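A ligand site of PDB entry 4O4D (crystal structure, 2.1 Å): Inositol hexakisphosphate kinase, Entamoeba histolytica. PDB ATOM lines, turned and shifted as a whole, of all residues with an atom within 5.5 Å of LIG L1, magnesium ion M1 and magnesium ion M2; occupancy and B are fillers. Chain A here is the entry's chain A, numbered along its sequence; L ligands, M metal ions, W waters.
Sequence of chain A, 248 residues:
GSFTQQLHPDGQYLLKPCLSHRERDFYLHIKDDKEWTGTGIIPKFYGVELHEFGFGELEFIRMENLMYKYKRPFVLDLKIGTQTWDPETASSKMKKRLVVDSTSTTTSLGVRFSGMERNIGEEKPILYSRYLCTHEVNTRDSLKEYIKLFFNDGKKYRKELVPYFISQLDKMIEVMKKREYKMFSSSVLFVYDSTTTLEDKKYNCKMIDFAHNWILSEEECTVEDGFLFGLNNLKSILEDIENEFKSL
An oxygen (O12) of LIG L1 is in hydrogen-bond range of the side-chain carboxylate of Asp 77, at 2.7 Å.
O of Glu 64 lies within hydrogen-bond range of N3 of LIG L1 (2.9 Å).
The side-chain sulfur (SD) of Met 63 lies within hydrogen-bond range of a nitrogen (N3) of LIG L1 (3.4 Å).
A nitrogen (N4) of LIG L1 lies within hydrogen-bond range of the backbone NH of Leu 66, 2.8 Å away.
O7 of LIG L1 is in salt-bridge range of NZ of Lys 16 (2.9 Å).
An oxygen (O2) of LG2 L2 lies within hydrogen-bond range of an oxygen (O3) of LIG L1, 2.6 Å away.
The side-chain carboxylate (OD1) of Asp 209 lies close to the side-chain amino group (NZ) of Lys 16.
N of Ile 208 is in hydrogen-bond range of O of Ser 187, 2.8 Å away.
N of Met 67 sits at hydrogen-bond distance from OD1 of Asn 65, 2.9 Å away.
OD1 of Asp 77 is in hydrogen-bond range of OG of Ser 187 (2.6 Å).
The side-chain amide nitrogen of Asn 65 lies close to the backbone carbonyl oxygen of Pro 9, at 3.4 Å.
The backbone carbonyl oxygen (O) of Met 63 sits at hydrogen-bond distance from the backbone NH (N) of Leu 14, at 2.9 Å.
The side-chain carboxylate (OE1) of Glu 23 lies within salt-bridge range of the side-chain amino group (NZ) of Lys 16, at 2.9 Å.
Leu 14 touches LIG L1 (CD2 to N2, 3.5 Å).
Pro 43 touches LIG L1 (CG to N3, 3.9 Å).
Asn 65 touches LIG L1.
Met 67 touches LIG L1.
Val 75 touches LIG L1.
CD1 of Leu 189 touches C4 of LIG L1, at 3.8 Å.
Ile 208 touches LIG L1.
Hydrophobic or aromatic side chains that line LIG L1: Leu 14, Pro 43, Met 63, Leu 66, Met 67, Val 75, Leu 189 and Ile 208.
The nearest printed residue that does not touch LIG L1 is Glu 23 (4.8 Å).
Within 4 Å of magnesium ion M1: Asp 209.
The nearest printed residue that does not touch magnesium ion M1 is Ser 185 (4.1 Å).
Within 4 Å of magnesium ion M2: Asp 209.
O1 of LIG L1 is bound to magnesium ion M1 (2.0 Å).
O8 of LIG L1 binds magnesium ion M1 (2.1 Å).
Magnesium ion M1 is bound by OD2 of Asp 209, 2.1 Å away.
Water W3 is bound to magnesium ion M1 (2.3 Å).
Magnesium ion M1 is bound by water W10, 2.3 Å away.
Magnesium ion M1 is bound by water W9.
Magnesium ion M1 has six donor atoms within binding distance.
An oxygen (O2) of LIG L1 is bound to magnesium ion M2 (1.9 Å).
O5 of LIG L1 is bound to magnesium ion M2 (2.0 Å).
Magnesium ion M2 is bound by water W5, at 2.0 Å.
The side-chain carboxylate (OD2) of Asp 209 is bound to magnesium ion M2 (2.2 Å).
Water W1 binds magnesium ion M2 (2.2 Å).
Magnesium ion M2 is bound by OD1 of Asp 209, 2.4 Å away.
Water W10 bridges OG of Ser 187 (2.6 Å) and O of Ser 185 (2.7 Å).
Water W9 lies within hydrogen-bond range of the side-chain amino group (NZ) of Lys 79 (3.0 Å) and the backbone carbonyl oxygen (O) of Ser 185 (3.1 Å).
Water W8 lies within hydrogen-bond range of O7 of LIG L1 (2.7 Å) and SD of Met 63 (3.8 Å).
Water W6 lies within hydrogen-bond range of O3 of LG2 L2 (2.5 Å), NZ of Lys 79 (3.0 Å) and O3 of LIG L1 (3.1 Å).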
ATOM      1  N   PRO A   9     -12.825  -6.123  -7.906  1.00  0.00           N
ATOM      2  CA  PRO A   9     -12.601  -4.971  -8.787  1.00  0.00           C
ATOM      3  C   PRO A   9     -13.600  -3.803  -8.601  1.00  0.00           C
ATOM      4  O   PRO A   9     -14.382  -3.485  -9.511  1.00  0.00           O
ATOM      5  CB  PRO A   9     -12.695  -5.599 -10.175  1.00  0.00           C
ATOM      6  CG  PRO A   9     -12.121  -6.974  -9.974  1.00  0.00           C
ATOM      7  CD  PRO A   9     -12.369  -7.377  -8.539  1.00  0.00           C
ATOM      8  N   LEU A  14      -5.680  -1.022  -8.534  1.00  0.00           N
ATOM      9  CA  LEU A  14      -5.199  -2.285  -7.956  1.00  0.00           C
ATOM     10  C   LEU A  14      -3.827  -1.987  -7.367  1.00  0.00           C
ATOM     11  O   LEU A  14      -2.972  -1.431  -8.048  1.00  0.00           O
ATOM     12  CB  LEU A  14      -5.087  -3.376  -9.055  1.00  0.00           C
ATOM     13  CG  LEU A  14      -4.259  -4.607  -8.768  1.00  0.00           C
ATOM     14  CD1 LEU A  14      -4.893  -5.399  -7.638  1.00  0.00           C
ATOM     15  CD2 LEU A  14      -4.171  -5.469 -10.016  1.00  0.00           C
ATOM     16  N   LYS A  16      -1.011  -3.930  -6.184  1.00  0.00           N
ATOM     17  CA  LYS A  16      -0.503  -5.318  -6.229  1.00  0.00           C
ATOM     18  C   LYS A  16       0.844  -5.443  -5.493  1.00  0.00           C
ATOM     19  O   LYS A  16       1.809  -4.763  -5.831  1.00  0.00           O
ATOM     20  CB  LYS A  16      -0.334  -5.747  -7.670  1.00  0.00           C
ATOM     21  CG  LYS A  16      -0.075  -7.241  -7.836  1.00  0.00           C
ATOM     22  CD  LYS A  16       0.190  -7.574  -9.283  1.00  0.00           C
ATOM     23  CE  LYS A  16       0.575  -9.054  -9.473  1.00  0.00           C
ATOM     24  NZ  LYS A  16       0.694  -9.343 -10.919  1.00  0.00           N
ATOM     25  N   GLU A  23       8.352  -8.031 -11.690  1.00  0.00           N
ATOM     26  CA  GLU A  23       7.215  -7.233 -12.181  1.00  0.00           C
ATOM     27  C   GLU A  23       7.480  -5.768 -12.009  1.00  0.00           C
ATOM     28  O   GLU A  23       7.314  -4.992 -12.960  1.00  0.00           O
ATOM     29  CB  GLU A  23       5.879  -7.609 -11.498  1.00  0.00           C
ATOM     30  CG  GLU A  23       4.673  -7.001 -12.262  1.00  0.00           C
ATOM     31  CD  GLU A  23       3.337  -7.615 -11.893  1.00  0.00           C
ATOM     32  OE1 GLU A  23       3.165  -7.918 -10.699  1.00  0.00           O
ATOM     33  OE2 GLU A  23       2.477  -7.808 -12.778  1.00  0.00           O
ATOM     34  N   PRO A  43      -1.782  -1.986 -18.296  1.00  0.00           N
ATOM     35  CA  PRO A  43      -2.452  -1.086 -17.337  1.00  0.00           C
ATOM     36  C   PRO A  43      -1.671   0.167 -17.080  1.00  0.00           C
ATOM     37  O   PRO A  43      -0.427   0.115 -17.108  1.00  0.00           O
ATOM     38  CB  PRO A  43      -2.517  -1.926 -16.065  1.00  0.00           C
ATOM     39  CG  PRO A  43      -2.492  -3.325 -16.557  1.00  0.00           C
ATOM     40  CD  PRO A  43      -1.550  -3.302 -17.701  1.00  0.00           C
ATOM     41  N   MET A  63      -1.503   0.373  -9.952  1.00  0.00           N
ATOM     42  CA  MET A  63      -1.954   0.488 -11.342  1.00  0.00           C
ATOM     43  C   MET A  63      -3.462   0.704 -11.418  1.00  0.00           C
ATOM     44  O   MET A  63      -4.149   0.556 -10.424  1.00  0.00           O
ATOM     45  CB  MET A  63      -1.555  -0.786 -12.105  1.00  0.00           C
ATOM     46  CG  MET A  63      -2.415  -2.000 -11.824  1.00  0.00           C
ATOM     47  SD  MET A  63      -1.855  -3.541 -12.630  1.00  0.00           S
ATOM     48  CE  MET A  63      -0.461  -3.966 -11.615  1.00  0.00           C
ATOM     49  N   GLU A  64      -3.987   1.030 -12.600  1.00  0.00           N
ATOM     50  CA  GLU A  64      -5.438   1.168 -12.722  1.00  0.00           C
ATOM     51  C   GLU A  64      -6.119  -0.207 -12.566  1.00  0.00           C
ATOM     52  O   GLU A  64      -5.580  -1.236 -12.944  1.00  0.00           O
ATOM     53  CB  GLU A  64      -5.857   1.836 -14.094  1.00  0.00           C
ATOM     54  CG  GLU A  64      -5.739   0.890 -15.296  1.00  0.00           C
ATOM     55  CD  GLU A  64      -6.021   1.460 -16.666  1.00  0.00           C
ATOM     56  OE1 GLU A  64      -5.108   1.388 -17.523  1.00  0.00           O
ATOM     57  OE2 GLU A  64      -7.146   1.913 -16.939  1.00  0.00           O
ATOM     58  N   ASN A  65      -7.318  -0.165 -12.031  1.00  0.00           N
ATOM     59  CA  ASN A  65      -8.254  -1.246 -12.047  1.00  0.00           C
ATOM     60  C   ASN A  65      -9.010  -1.116 -13.363  1.00  0.00           C
ATOM     61  O   ASN A  65      -9.765  -0.145 -13.563  1.00  0.00           O
ATOM     62  CB  ASN A  65      -9.252  -1.089 -10.900  1.00  0.00           C
ATOM     63  CG  ASN A  65     -10.418  -2.078 -10.993  1.00  0.00           C
ATOM     64  OD1 ASN A  65     -10.427  -2.991 -11.814  1.00  0.00           O
ATOM     65  ND2 ASN A  65     -11.418  -1.888 -10.136  1.00  0.00           N
ATOM     66  N   LEU A  66      -8.795  -2.055 -14.264  1.00  0.00           N
ATOM     67  CA  LEU A  66      -9.381  -1.970 -15.603  1.00  0.00           C
ATOM     68  C   LEU A  66     -10.914  -2.095 -15.584  1.00  0.00           C
ATOM     69  O   LEU A  66     -11.581  -1.698 -16.555  1.00  0.00           O
ATOM     70  CB  LEU A  66      -8.776  -3.034 -16.552  1.00  0.00           C
ATOM     71  CG  LEU A  66      -7.260  -3.038 -16.706  1.00  0.00           C
ATOM     72  CD1 LEU A  66      -6.846  -4.398 -17.274  1.00  0.00           C
ATOM     73  CD2 LEU A  66      -6.754  -1.858 -17.527  1.00  0.00           C
ATOM     74  N   MET A  67     -11.481  -2.585 -14.496  1.00  0.00           N
ATOM     75  CA  MET A  67     -12.944  -2.670 -14.406  1.00  0.00           C
ATOM     76  C   MET A  67     -13.604  -1.639 -13.515  1.00  0.00           C
ATOM     77  O   MET A  67     -14.728  -1.813 -13.127  1.00  0.00           O
ATOM     78  CB  MET A  67     -13.337  -4.069 -13.954  1.00  0.00           C
ATOM     79  CG  MET A  67     -13.023  -5.106 -15.027  1.00  0.00           C
ATOM     80  SD  MET A  67     -13.442  -6.764 -14.493  1.00  0.00           S
ATOM     81  CE  MET A  67     -11.916  -7.236 -13.675  1.00  0.00           C
ATOM     82  N   VAL A  75     -15.165 -10.967 -18.003  1.00  0.00           N
ATOM     83  CA  VAL A  75     -13.703 -11.096 -17.809  1.00  0.00           C
ATOM     84  C   VAL A  75     -13.234 -12.398 -18.409  1.00  0.00           C
ATOM     85  O   VAL A  75     -13.820 -13.446 -18.109  1.00  0.00           O
ATOM     86  CB  VAL A  75     -13.348 -11.100 -16.303  1.00  0.00           C
ATOM     87  CG1 VAL A  75     -11.822 -11.109 -16.119  1.00  0.00           C
ATOM     88  CG2 VAL A  75     -13.954  -9.895 -15.599  1.00  0.00           C
ATOM     89  N   ASP A  77      -9.370 -14.341 -19.010  1.00  0.00           N
ATOM     90  CA  ASP A  77      -7.920 -14.349 -18.851  1.00  0.00           C
ATOM     91  C   ASP A  77      -7.353 -15.425 -19.767  1.00  0.00           C
ATOM     92  O   ASP A  77      -7.700 -16.613 -19.657  1.00  0.00           O
ATOM     93  CB  ASP A  77      -7.557 -14.617 -17.403  1.00  0.00           C
ATOM     94  CG  ASP A  77      -6.059 -14.459 -17.128  1.00  0.00           C
ATOM     95  OD1 ASP A  77      -5.264 -15.150 -17.796  1.00  0.00           O
ATOM     96  OD2 ASP A  77      -5.640 -13.633 -16.270  1.00  0.00           O
ATOM     97  N   LYS A  79      -3.743 -17.009 -20.990  1.00  0.00           N
ATOM     98  CA  LYS A  79      -2.342 -17.062 -20.629  1.00  0.00           C
ATOM     99  C   LYS A  79      -1.552 -17.288 -21.908  1.00  0.00           C
ATOM    100  O   LYS A  79      -1.891 -18.177 -22.719  1.00  0.00           O
ATOM    101  CB  LYS A  79      -2.123 -18.160 -19.624  1.00  0.00           C
ATOM    102  CG  LYS A  79      -0.742 -18.164 -19.004  1.00  0.00           C
ATOM    103  CD  LYS A  79      -0.722 -18.987 -17.719  1.00  0.00           C
ATOM    104  CE  LYS A  79      -1.500 -18.250 -16.633  1.00  0.00           C
ATOM    105  NZ  LYS A  79      -1.235 -18.818 -15.286  1.00  0.00           N
ATOM    106  N   SER A 185       4.158 -16.868 -18.256  1.00  0.00           N
ATOM    107  CA  SER A 185       2.911 -16.915 -17.444  1.00  0.00           C
ATOM    108  C   SER A 185       2.157 -15.598 -17.361  1.00  0.00           C
ATOM    109  O   SER A 185       1.270 -15.432 -16.521  1.00  0.00           O
ATOM    110  CB  SER A 185       3.170 -17.485 -16.052  1.00  0.00           C
ATOM    111  OG  SER A 185       3.634 -18.819 -16.185  1.00  0.00           O
ATOM    112  N   SER A 187      -0.480 -12.809 -19.110  1.00  0.00           N
ATOM    113  CA  SER A 187      -1.747 -12.995 -19.794  1.00  0.00           C
ATOM    114  C   SER A 187      -2.144 -11.818 -20.624  1.00  0.00           C
ATOM    115  O   SER A 187      -1.640 -10.708 -20.394  1.00  0.00           O
ATOM    116  CB  SER A 187      -2.880 -13.246 -18.780  1.00  0.00           C
ATOM    117  OG  SER A 187      -2.757 -14.487 -18.163  1.00  0.00           O
ATOM    118  N   LEU A 189      -5.634  -9.953 -20.822  1.00  0.00           N
ATOM    119  CA  LEU A 189      -6.892  -9.858 -20.150  1.00  0.00           C
ATOM    120  C   LEU A 189      -7.944  -9.121 -21.022  1.00  0.00           C
ATOM    121  O   LEU A 189      -7.707  -7.965 -21.425  1.00  0.00           O
ATOM    122  CB  LEU A 189      -6.698  -9.120 -18.812  1.00  0.00           C
ATOM    123  CG  LEU A 189      -7.951  -9.042 -17.932  1.00  0.00           C
ATOM    124  CD1 LEU A 189      -8.258 -10.419 -17.380  1.00  0.00           C
ATOM    125  CD2 LEU A 189      -7.729  -8.033 -16.808  1.00  0.00           C
ATOM    126  N   ILE A 208      -1.014  -8.374 -18.909  1.00  0.00           N
ATOM    127  CA  ILE A 208      -0.843  -8.286 -17.487  1.00  0.00           C
ATOM    128  C   ILE A 208       0.046  -9.380 -16.924  1.00  0.00           C
ATOM    129  O   ILE A 208       0.300 -10.405 -17.576  1.00  0.00           O
ATOM    130  CB  ILE A 208      -2.178  -8.376 -16.746  1.00  0.00           C
ATOM    131  CG1 ILE A 208      -2.934  -9.613 -17.143  1.00  0.00           C
ATOM    132  CG2 ILE A 208      -3.042  -7.135 -16.993  1.00  0.00           C
ATOM    133  CD1 ILE A 208      -3.848 -10.086 -16.059  1.00  0.00           C
ATOM    134  N   ASP A 209       0.476  -9.158 -15.675  1.00  0.00           N
ATOM    135  CA  ASP A 209       1.181 -10.131 -14.853  1.00  0.00           C
ATOM    136  C   ASP A 209       2.568 -10.448 -15.293  1.00  0.00           C
ATOM    137  O   ASP A 209       2.807 -11.454 -16.012  1.00  0.00           O
ATOM    138  CB  ASP A 209       0.407 -11.425 -14.699  1.00  0.00           C
ATOM    139  CG  ASP A 209       0.924 -12.274 -13.597  1.00  0.00           C
ATOM    140  OD1 ASP A 209       1.947 -11.891 -12.908  1.00  0.00           O
ATOM    141  OD2 ASP A 209       0.312 -13.352 -13.385  1.00  0.00           O
ATOM    142  N   ALA A 211       5.383 -10.889 -13.450  1.00  0.00           N
ATOM    143  CA  ALA A 211       6.171 -11.482 -12.391  1.00  0.00           C
ATOM    144  C   ALA A 211       7.288 -12.400 -12.885  1.00  0.00           C
ATOM    145  O   ALA A 211       8.206 -12.704 -12.140  1.00  0.00           O
ATOM    146  CB  ALA A 211       5.240 -12.254 -11.465  1.00  0.00           C
HETATM  147  P1  LIG L   1      -1.272 -15.313 -10.898  1.00  0.00           P
HETATM  148  O1  LIG L   1      -2.047 -15.163 -12.184  1.00  0.00           O
HETATM  149  O2  LIG L   1       0.227 -15.208 -11.106  1.00  0.00           O
HETATM  150  O3  LIG L   1      -1.695 -16.506 -10.062  1.00  0.00           O
HETATM  151  P2  LIG L   1      -1.267 -12.598  -9.890  1.00  0.00           P
HETATM  152  O4  LIG L   1      -1.296 -12.090  -8.457  1.00  0.00           O
HETATM  153  O5  LIG L   1       0.037 -12.333 -10.625  1.00  0.00           O
HETATM  154  O6  LIG L   1      -1.769 -14.106  -9.935  1.00  0.00           O
HETATM  155  P3  LIG L   1      -2.520 -11.294 -12.128  1.00  0.00           P
HETATM  156  O7  LIG L   1      -1.751 -10.003 -12.311  1.00  0.00           O
HETATM  157  O8  LIG L   1      -2.304 -12.413 -13.116  1.00  0.00           O
HETATM  158  O9  LIG L   1      -2.473 -11.790 -10.596  1.00  0.00           O
HETATM  159  O10 LIG L   1      -4.087 -10.977 -12.092  1.00  0.00           O
HETATM  160  C1  LIG L   1      -5.030 -12.012 -11.741  1.00  0.00           C
HETATM  161  C2  LIG L   1      -6.443 -11.555 -12.093  1.00  0.00           C
HETATM  162  O11 LIG L   1      -6.724 -10.265 -11.519  1.00  0.00           O
HETATM  163  C3  LIG L   1      -6.618 -11.377 -13.578  1.00  0.00           C
HETATM  164  O12 LIG L   1      -7.037 -12.587 -14.212  1.00  0.00           O
HETATM  165  C4  LIG L   1      -7.673 -10.335 -13.649  1.00  0.00           C
HETATM  166  O13 LIG L   1      -8.924 -10.952 -13.508  1.00  0.00           O
HETATM  167  C5  LIG L   1      -7.446  -9.440 -12.455  1.00  0.00           C
HETATM  168  N1  LIG L   1      -6.626  -8.234 -12.764  1.00  0.00           N
HETATM  169  C6  LIG L   1      -5.297  -8.231 -12.831  1.00  0.00           C
HETATM  170  N2  LIG L   1      -4.831  -7.000 -13.146  1.00  0.00           N
HETATM  171  C7  LIG L   1      -5.921  -6.206 -13.237  1.00  0.00           C
HETATM  172  C8  LIG L   1      -6.128  -4.787 -13.478  1.00  0.00           C
HETATM  173  N3  LIG L   1      -5.092  -3.984 -13.721  1.00  0.00           N
HETATM  174  N4  LIG L   1      -7.386  -4.357 -13.500  1.00  0.00           N
HETATM  175  C9  LIG L   1      -8.443  -5.183 -13.302  1.00  0.00           C
HETATM  176  N5  LIG L   1      -8.345  -6.488 -13.053  1.00  0.00           N
HETATM  177  C10 LIG L   1      -7.094  -7.028 -12.992  1.00  0.00           C
HETATM  178  C1  LG2 L   2       1.641 -19.657  -9.900  1.00  0.00           C
HETATM  179  C2  LG2 L   2       0.299 -19.180 -10.459  1.00  0.00           C
HETATM  180  C3  LG2 L   2      -0.307 -20.358 -11.208  1.00  0.00           C
HETATM  181  C4  LG2 L   2      -0.550 -21.488 -10.223  1.00  0.00           C
HETATM  182  C5  LG2 L   2       0.786 -21.924  -9.656  1.00  0.00           C
HETATM  183  C6  LG2 L   2       1.498 -20.793  -8.924  1.00  0.00           C
HETATM  184  O1  LG2 L   2       2.311 -18.573  -9.296  1.00  0.00           O
HETATM  185  O2  LG2 L   2      -0.511 -18.709  -9.371  1.00  0.00           O
HETATM  186  O3  LG2 L   2      -1.507 -19.990 -11.889  1.00  0.00           O
HETATM  187  O4  LG2 L   2      -1.168 -22.617 -10.855  1.00  0.00           O
HETATM  188  O5  LG2 L   2       0.561 -23.032  -8.813  1.00  0.00           O
HETATM  189  O6  LG2 L   2       2.803 -21.228  -8.539  1.00  0.00           O
HETATM  190  P1  LG2 L   2       3.622 -18.028 -10.047  1.00  0.00           P
HETATM  191  O7  LG2 L   2       3.223 -17.998 -11.525  1.00  0.00           O
HETATM  192  O8  LG2 L   2       4.588 -19.099  -9.586  1.00  0.00           O
HETATM  193  O9  LG2 L   2       3.891 -16.634  -9.497  1.00  0.00           O
HETATM  194  P2  LG2 L   2      -2.706 -23.046 -10.580  1.00  0.00           P
HETATM  195  O10 LG2 L   2      -2.825 -24.497 -10.984  1.00  0.00           O
HETATM  196  O11 LG2 L   2      -3.505 -22.079 -11.440  1.00  0.00           O
HETATM  197  O12 LG2 L   2      -2.844 -22.906  -9.090  1.00  0.00           O
HETATM  198  P3  LG2 L   2       1.506 -24.335  -8.864  1.00  0.00           P
HETATM  199  O13 LG2 L   2       1.982 -24.549 -10.286  1.00  0.00           O
HETATM  200  O14 LG2 L   2       0.526 -25.386  -8.420  1.00  0.00           O
HETATM  201  O15 LG2 L   2       2.609 -23.961  -7.914  1.00  0.00           O
HETATM  202 MG    MG M   1      -1.555 -14.252 -13.856  1.00  0.00          MG
HETATM  203 MG    MG M   2       1.298 -13.646 -11.456  1.00  0.00          MG
HETATM  204  O   HOH W   1       2.688 -14.871 -12.620  1.00  0.00           O
HETATM  205  O   HOH W   2      -4.599 -17.902  -9.760  1.00  0.00           O
HETATM  206  O   HOH W   3      -3.538 -15.090 -14.511  1.00  0.00           O
HETATM  207  O   HOH W   4      -5.997 -14.045  -9.222  1.00  0.00           O
HETATM  208  O   HOH W   5       2.717 -13.425 -10.007  1.00  0.00           O
HETATM  209  O   HOH W   6      -2.526 -17.814 -12.737  1.00  0.00           O
HETATM  210  O   HOH W   7      -4.686 -15.386 -11.743  1.00  0.00           O
HETATM  211  O   HOH W   8      -1.886  -7.332 -12.851  1.00  0.00           O
HETATM  212  O   HOH W   9      -0.375 -16.233 -14.067  1.00  0.00           O
HETATM  213  O   HOH W  10      -1.149 -14.258 -16.080  1.00  0.00           O
HETATM  214  O   HOH W  11      -4.311 -12.693  -7.941  1.00  0.00           O
HETATM  215  O   HOH W  12      -0.277 -11.014  -5.574  1.00  0.00           O
